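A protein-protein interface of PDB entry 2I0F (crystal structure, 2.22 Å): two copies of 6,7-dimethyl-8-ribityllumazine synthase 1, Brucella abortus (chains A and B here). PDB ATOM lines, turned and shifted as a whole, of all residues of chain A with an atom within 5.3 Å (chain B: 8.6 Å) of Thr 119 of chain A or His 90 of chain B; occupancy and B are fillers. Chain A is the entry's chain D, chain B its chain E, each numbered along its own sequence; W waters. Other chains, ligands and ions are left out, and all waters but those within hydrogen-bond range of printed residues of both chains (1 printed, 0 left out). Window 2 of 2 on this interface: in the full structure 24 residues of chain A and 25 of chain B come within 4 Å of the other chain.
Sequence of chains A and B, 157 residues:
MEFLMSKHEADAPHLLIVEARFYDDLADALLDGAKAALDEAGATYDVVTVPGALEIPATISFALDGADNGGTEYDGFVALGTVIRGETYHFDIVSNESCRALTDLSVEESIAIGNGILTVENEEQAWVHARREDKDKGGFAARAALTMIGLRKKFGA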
ATOM      1  N   VAL A  83      27.688   2.950   2.128  1.00  0.00           N
ATOM      2  CA  VAL A  83      27.150   1.825   2.874  1.00  0.00           C
ATOM      3  C   VAL A  83      25.772   2.185   3.413  1.00  0.00           C
ATOM      4  O   VAL A  83      25.640   2.850   4.440  1.00  0.00           O
ATOM      5  CB  VAL A  83      28.081   1.441   4.040  1.00  0.00           C
ATOM      6  CG1 VAL A  83      27.546   0.211   4.744  1.00  0.00           C
ATOM      7  CG2 VAL A  83      29.490   1.186   3.518  1.00  0.00           C
ATOM      8  N   SER A  95      30.297  -0.705   8.007  1.00  0.00           N
ATOM      9  CA  SER A  95      30.409   0.711   8.302  1.00  0.00           C
ATOM     10  C   SER A  95      31.357   0.971   9.472  1.00  0.00           C
ATOM     11  O   SER A  95      32.291   1.767   9.360  1.00  0.00           O
ATOM     12  CB  SER A  95      29.029   1.287   8.601  1.00  0.00           C
ATOM     13  OG  SER A  95      29.076   2.701   8.571  1.00  0.00           O
ATOM     14  N   ASN A 115      38.300  10.752   5.099  1.00  0.00           N
ATOM     15  CA  ASN A 115      37.300   9.706   5.182  1.00  0.00           C
ATOM     16  C   ASN A 115      36.041  10.076   4.417  1.00  0.00           C
ATOM     17  O   ASN A 115      35.220  10.859   4.897  1.00  0.00           O
ATOM     18  CB  ASN A 115      36.949   9.427   6.641  1.00  0.00           C
ATOM     19  CG  ASN A 115      36.259   8.106   6.815  1.00  0.00           C
ATOM     20  OD1 ASN A 115      35.462   7.702   5.973  1.00  0.00           O
ATOM     21  ND2 ASN A 115      36.560   7.415   7.910  1.00  0.00           N
ATOM     22  N   ILE A 117      33.820   7.713   3.287  1.00  0.00           N
ATOM     23  CA  ILE A 117      32.973   6.534   3.271  1.00  0.00           C
ATOM     24  C   ILE A 117      31.617   6.930   3.835  1.00  0.00           C
ATOM     25  O   ILE A 117      31.488   7.182   5.033  1.00  0.00           O
ATOM     26  CB  ILE A 117      33.584   5.395   4.115  1.00  0.00           C
ATOM     27  CG1 ILE A 117      34.869   4.893   3.445  1.00  0.00           C
ATOM     28  CG2 ILE A 117      32.584   4.262   4.262  1.00  0.00           C
ATOM     29  CD1 ILE A 117      35.554   3.752   4.173  1.00  0.00           C
ATOM     30  N   LEU A 118      30.617   6.993   2.960  1.00  0.00           N
ATOM     31  CA  LEU A 118      29.263   7.379   3.353  1.00  0.00           C
ATOM     32  C   LEU A 118      28.459   6.255   3.968  1.00  0.00           C
ATOM     33  O   LEU A 118      28.444   5.138   3.465  1.00  0.00           O
ATOM     34  CB  LEU A 118      28.478   7.916   2.153  1.00  0.00           C
ATOM     35  CG  LEU A 118      29.035   9.107   1.382  1.00  0.00           C
ATOM     36  CD1 LEU A 118      27.937   9.679   0.491  1.00  0.00           C
ATOM     37  CD2 LEU A 118      29.530  10.164   2.354  1.00  0.00           C
ATOM     38  N   THR A 119      27.771   6.574   5.055  1.00  0.00           N
ATOM     39  CA  THR A 119      26.934   5.612   5.747  1.00  0.00           C
ATOM     40  C   THR A 119      25.554   6.236   5.891  1.00  0.00           C
ATOM     41  O   THR A 119      25.282   6.938   6.864  1.00  0.00           O
ATOM     42  CB  THR A 119      27.484   5.299   7.141  1.00  0.00           C
ATOM     43  OG1 THR A 119      28.848   4.874   7.034  1.00  0.00           O
ATOM     44  CG2 THR A 119      26.665   4.202   7.796  1.00  0.00           C
ATOM     45  N   VAL A 120      24.690   5.990   4.912  1.00  0.00           N
ATOM     46  CA  VAL A 120      23.340   6.539   4.928  1.00  0.00           C
ATOM     47  C   VAL A 120      22.301   5.479   5.274  1.00  0.00           C
ATOM     48  O   VAL A 120      22.635   4.315   5.499  1.00  0.00           O
ATOM     49  CB  VAL A 120      22.979   7.163   3.565  1.00  0.00           C
ATOM     50  CG1 VAL A 120      23.920   8.316   3.263  1.00  0.00           C
ATOM     51  CG2 VAL A 120      23.062   6.112   2.471  1.00  0.00           C
ATOM     52  N   GLU A 121      21.037   5.889   5.309  1.00  0.00           N
ATOM     53  CA  GLU A 121      19.958   4.972   5.639  1.00  0.00           C
ATOM     54  C   GLU A 121      19.252   4.455   4.391  1.00  0.00           C
ATOM     55  O   GLU A 121      18.648   3.381   4.413  1.00  0.00           O
ATOM     56  CB  GLU A 121      18.944   5.663   6.548  1.00  0.00           C
ATOM     57  CG  GLU A 121      18.174   4.700   7.427  1.00  0.00           C
ATOM     58  CD  GLU A 121      19.074   3.996   8.421  1.00  0.00           C
ATOM     59  OE1 GLU A 121      19.662   4.684   9.280  1.00  0.00           O
ATOM     60  OE2 GLU A 121      19.199   2.757   8.342  1.00  0.00           O
ATOM     61  N   GLY B  52      37.066  16.880  11.467  1.00  0.00           N
ATOM     62  CA  GLY B  52      36.192  16.115  12.333  1.00  0.00           C
ATOM     63  C   GLY B  52      36.863  15.395  13.486  1.00  0.00           C
ATOM     64  O   GLY B  52      38.087  15.299  13.568  1.00  0.00           O
ATOM     65  N   ALA B  53      36.034  14.891  14.386  1.00  0.00           N
ATOM     66  CA  ALA B  53      36.499  14.171  15.554  1.00  0.00           C
ATOM     67  C   ALA B  53      37.403  13.010  15.152  1.00  0.00           C
ATOM     68  O   ALA B  53      38.391  12.731  15.818  1.00  0.00           O
ATOM     69  CB  ALA B  53      35.298  13.660  16.343  1.00  0.00           C
ATOM     70  N   LEU B  54      37.080  12.348  14.046  1.00  0.00           N
ATOM     71  CA  LEU B  54      37.878  11.220  13.599  1.00  0.00           C
ATOM     72  C   LEU B  54      39.315  11.555  13.207  1.00  0.00           C
ATOM     73  O   LEU B  54      40.161  10.662  13.170  1.00  0.00           O
ATOM     74  CB  LEU B  54      37.181  10.497  12.442  1.00  0.00           C
ATOM     75  CG  LEU B  54      35.880   9.773  12.803  1.00  0.00           C
ATOM     76  CD1 LEU B  54      35.362   9.032  11.582  1.00  0.00           C
ATOM     77  CD2 LEU B  54      36.123   8.799  13.948  1.00  0.00           C
ATOM     78  N   GLU B  55      39.604  12.820  12.912  1.00  0.00           N
ATOM     79  CA  GLU B  55      40.971  13.192  12.547  1.00  0.00           C
ATOM     80  C   GLU B  55      41.786  13.674  13.739  1.00  0.00           C
ATOM     81  O   GLU B  55      42.959  14.028  13.591  1.00  0.00           O
ATOM     82  CB  GLU B  55      40.992  14.288  11.474  1.00  0.00           C
ATOM     83  CG  GLU B  55      40.539  13.845  10.095  1.00  0.00           C
ATOM     84  CD  GLU B  55      39.033  13.716   9.990  1.00  0.00           C
ATOM     85  OE1 GLU B  55      38.329  14.606  10.498  1.00  0.00           O
ATOM     86  OE2 GLU B  55      38.551  12.737   9.389  1.00  0.00           O
ATOM     87  N   VAL B  83      29.770  16.216  18.273  1.00  0.00           N
ATOM     88  CA  VAL B  83      29.041  15.275  17.440  1.00  0.00           C
ATOM     89  C   VAL B  83      27.569  15.339  17.822  1.00  0.00           C
ATOM     90  O   VAL B  83      27.194  15.014  18.946  1.00  0.00           O
ATOM     91  CB  VAL B  83      29.556  13.842  17.650  1.00  0.00           C
ATOM     92  CG1 VAL B  83      28.748  12.872  16.795  1.00  0.00           C
ATOM     93  CG2 VAL B  83      31.048  13.775  17.311  1.00  0.00           C
ATOM     94  N   ILE B  84      26.738  15.773  16.888  1.00  0.00           N
ATOM     95  CA  ILE B  84      25.315  15.888  17.152  1.00  0.00           C
ATOM     96  C   ILE B  84      24.575  14.777  16.430  1.00  0.00           C
ATOM     97  O   ILE B  84      24.602  14.712  15.203  1.00  0.00           O
ATOM     98  CB  ILE B  84      24.781  17.273  16.682  1.00  0.00           C
ATOM     99  CG1 ILE B  84      25.569  18.392  17.369  1.00  0.00           C
ATOM    100  CG2 ILE B  84      23.288  17.402  16.993  1.00  0.00           C
ATOM    101  CD1 ILE B  84      25.074  19.793  17.046  1.00  0.00           C
ATOM    102  N   ARG B  85      23.928  13.894  17.185  1.00  0.00           N
ATOM    103  CA  ARG B  85      23.188  12.803  16.569  1.00  0.00           C
ATOM    104  C   ARG B  85      22.091  13.366  15.677  1.00  0.00           C
ATOM    105  O   ARG B  85      20.957  13.560  16.116  1.00  0.00           O
ATOM    106  CB  ARG B  85      22.570  11.892  17.628  1.00  0.00           C
ATOM    107  CG  ARG B  85      21.719  10.790  17.020  1.00  0.00           C
ATOM    108  CD  ARG B  85      21.279   9.759  18.037  1.00  0.00           C
ATOM    109  NE  ARG B  85      20.463   8.723  17.410  1.00  0.00           N
ATOM    110  CZ  ARG B  85      19.991   7.655  18.042  1.00  0.00           C
ATOM    111  NH1 ARG B  85      20.253   7.474  19.330  1.00  0.00           N
ATOM    112  NH2 ARG B  85      19.255   6.766  17.388  1.00  0.00           N
ATOM    113  N   GLY B  86      22.443  13.632  14.423  1.00  0.00           N
ATOM    114  CA  GLY B  86      21.485  14.177  13.480  1.00  0.00           C
ATOM    115  C   GLY B  86      20.552  13.119  12.931  1.00  0.00           C
ATOM    116  O   GLY B  86      20.167  12.191  13.643  1.00  0.00           O
ATOM    117  N   GLU B  87      20.190  13.255  11.660  1.00  0.00           N
ATOM    118  CA  GLU B  87      19.290  12.308  11.014  1.00  0.00           C
ATOM    119  C   GLU B  87      20.049  11.133  10.407  1.00  0.00           C
ATOM    120  O   GLU B  87      19.527  10.019  10.329  1.00  0.00           O
ATOM    121  CB  GLU B  87      18.482  13.019   9.927  1.00  0.00           C
ATOM    122  CG  GLU B  87      17.655  14.180  10.445  1.00  0.00           C
ATOM    123  CD  GLU B  87      16.914  14.905   9.342  1.00  0.00           C
ATOM    124  OE1 GLU B  87      17.578  15.399   8.406  1.00  0.00           O
ATOM    125  OE2 GLU B  87      15.668  14.982   9.412  1.00  0.00           O
ATOM    126  N   THR B  88      21.281  11.386   9.979  1.00  0.00           N
ATOM    127  CA  THR B  88      22.110  10.349   9.376  1.00  0.00           C
ATOM    128  C   THR B  88      22.678   9.410  10.435  1.00  0.00           C
ATOM    129  O   THR B  88      22.787   9.769  11.608  1.00  0.00           O
ATOM    130  CB  THR B  88      23.275  10.968   8.574  1.00  0.00           C
ATOM    131  OG1 THR B  88      22.748  11.829   7.557  1.00  0.00           O
ATOM    132  CG2 THR B  88      24.116   9.880   7.919  1.00  0.00           C
ATOM    133  N   TYR B  89      23.033   8.200  10.012  1.00  0.00           N
ATOM    134  CA  TYR B  89      23.588   7.198  10.913  1.00  0.00           C
ATOM    135  C   TYR B  89      25.077   7.442  11.126  1.00  0.00           C
ATOM    136  O   TYR B  89      25.695   6.853  12.014  1.00  0.00           O
ATOM    137  CB  TYR B  89      23.381   5.800  10.325  1.00  0.00           C
ATOM    138  CG  TYR B  89      22.710   4.827  11.266  1.00  0.00           C
ATOM    139  CD1 TYR B  89      21.413   5.055  11.725  1.00  0.00           C
ATOM    140  CD2 TYR B  89      23.368   3.675  11.695  1.00  0.00           C
ATOM    141  CE1 TYR B  89      20.786   4.159  12.588  1.00  0.00           C
ATOM    142  CE2 TYR B  89      22.751   2.773  12.558  1.00  0.00           C
ATOM    143  CZ  TYR B  89      21.461   3.021  13.000  1.00  0.00           C
ATOM    144  OH  TYR B  89      20.845   2.137  13.856  1.00  0.00           O
ATOM    145  N   HIS B  90      25.648   8.315  10.304  1.00  0.00           N
ATOM    146  CA  HIS B  90      27.068   8.628  10.387  1.00  0.00           C
ATOM    147  C   HIS B  90      27.363   9.592  11.532  1.00  0.00           C
ATOM    148  O   HIS B  90      27.787  10.726  11.307  1.00  0.00           O
ATOM    149  CB  HIS B  90      27.546   9.232   9.063  1.00  0.00           C
ATOM    150  CG  HIS B  90      29.035   9.341   8.948  1.00  0.00           C
ATOM    151  ND1 HIS B  90      29.806  10.028   9.861  1.00  0.00           N
ATOM    152  CD2 HIS B  90      29.894   8.854   8.022  1.00  0.00           C
ATOM    153  CE1 HIS B  90      31.075   9.962   9.502  1.00  0.00           C
ATOM    154  NE2 HIS B  90      31.156   9.255   8.389  1.00  0.00           N
ATOM    155  N   PHE B  91      27.126   9.136  12.759  1.00  0.00           N
ATOM    156  CA  PHE B  91      27.382   9.946  13.946  1.00  0.00           C
ATOM    157  C   PHE B  91      27.755   9.052  15.122  1.00  0.00           C
ATOM    158  O   PHE B  91      28.691   9.347  15.866  1.00  0.00           O
ATOM    159  CB  PHE B  91      26.157  10.797  14.306  1.00  0.00           C
ATOM    160  CG  PHE B  91      25.848  11.873  13.299  1.00  0.00           C
ATOM    161  CD1 PHE B  91      24.942  11.644  12.269  1.00  0.00           C
ATOM    162  CD2 PHE B  91      26.485  13.109  13.366  1.00  0.00           C
ATOM    163  CE1 PHE B  91      24.674  12.628  11.319  1.00  0.00           C
ATOM    164  CE2 PHE B  91      26.224  14.099  12.420  1.00  0.00           C
ATOM    165  CZ  PHE B  91      25.317  13.858  11.396  1.00  0.00           C
ATOM    166  N   ASP B  92      27.022   7.955  15.283  1.00  0.00           N
ATOM    167  CA  ASP B  92      27.297   7.012  16.358  1.00  0.00           C
ATOM    168  C   ASP B  92      28.654   6.377  16.097  1.00  0.00           C
ATOM    169  O   ASP B  92      29.351   5.963  17.024  1.00  0.00           O
ATOM    170  CB  ASP B  92      26.213   5.933  16.419  1.00  0.00           C
ATOM    171  CG  ASP B  92      24.853   6.500  16.782  1.00  0.00           C
ATOM    172  OD1 ASP B  92      24.748   7.165  17.837  1.00  0.00           O
ATOM    173  OD2 ASP B  92      23.889   6.280  16.015  1.00  0.00           O
ATOM    174  N   ILE B  93      29.015   6.298  14.822  1.00  0.00           N
ATOM    175  CA  ILE B  93      30.300   5.742  14.418  1.00  0.00           C
ATOM    176  C   ILE B  93      31.412   6.690  14.867  1.00  0.00           C
ATOM    177  O   ILE B  93      32.386   6.271  15.490  1.00  0.00           O
ATOM    178  CB  ILE B  93      30.375   5.572  12.881  1.00  0.00           C
ATOM    179  CG1 ILE B  93      29.474   4.418  12.442  1.00  0.00           C
ATOM    180  CG2 ILE B  93      31.804   5.327  12.444  1.00  0.00           C
ATOM    181  CD1 ILE B  93      29.478   4.187  10.943  1.00  0.00           C
ATOM    182  N   VAL B  94      31.253   7.969  14.546  1.00  0.00           N
ATOM    183  CA  VAL B  94      32.237   8.977  14.914  1.00  0.00           C
ATOM    184  C   VAL B  94      32.405   9.037  16.431  1.00  0.00           C
ATOM    185  O   VAL B  94      33.511   9.202  16.944  1.00  0.00           O
ATOM    186  CB  VAL B  94      31.821  10.369  14.399  1.00  0.00           C
ATOM    187  CG1 VAL B  94      32.866  11.394  14.777  1.00  0.00           C
ATOM    188  CG2 VAL B  94      31.636  10.333  12.893  1.00  0.00           C
ATOM    189  N   SER B  95      31.300   8.897  17.147  1.00  0.00           N
ATOM    190  CA  SER B  95      31.339   8.939  18.600  1.00  0.00           C
ATOM    191  C   SER B  95      32.182   7.788  19.167  1.00  0.00           C
ATOM    192  O   SER B  95      33.114   8.011  19.940  1.00  0.00           O
ATOM    193  CB  SER B  95      29.915   8.873  19.147  1.00  0.00           C
ATOM    194  OG  SER B  95      29.925   8.812  20.557  1.00  0.00           O
HETATM  195  O   HOH W   1      38.083  13.057   6.761  1.00  0.00           O
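Ser 95 of chain A touches Ile 93 of chain B. O of Ile 117 of chain A touches CD2 of His 90 of chain B, 3.8 Å away. O of Thr 119 of chain A touches CG2 of Thr 88 of chain B (3.3 Å). N of His 90 of chain B touches O of Thr 119 of chain A, 3.7 Å away. Tyr 89 of chain B touches Glu 121 of chain A (CD1 to OE1, 3.0 Å).
Printed residues of chain B within 4 Å of Thr 119 of chain A: Thr 88 (3.3 Å) and His 90 (3.7 Å). His 90 of chain B touches just these residues of chain A: Ile 117 and Thr 119. No residue of chain B comes within 4 Å of Val 120 of chain A. Printed residues of chain B within 4 Å of Ser 95 of chain A: Ile 93. Printed residues of chain A within 4 Å of Thr 88 of chain B: Thr 119.
The side-chain hydroxyl of Ser 95 of chain A sits at hydrogen-bond distance from the side-chain hydroxyl of Thr 119 of chain A. N of Ile 117 of chain A sits at hydrogen-bond distance from OD1 of Asn 115 of chain A, 3.1 Å away.
2 positions are printed for both chains.
Among the printed residues, 5 pairs touch across the chains.
Water W1 lies within hydrogen-bond range of the side-chain carboxylate of Glu 55 of chain B (2.7 Å) and the backbone NH of Asn 115 of chain A (2.8 Å).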
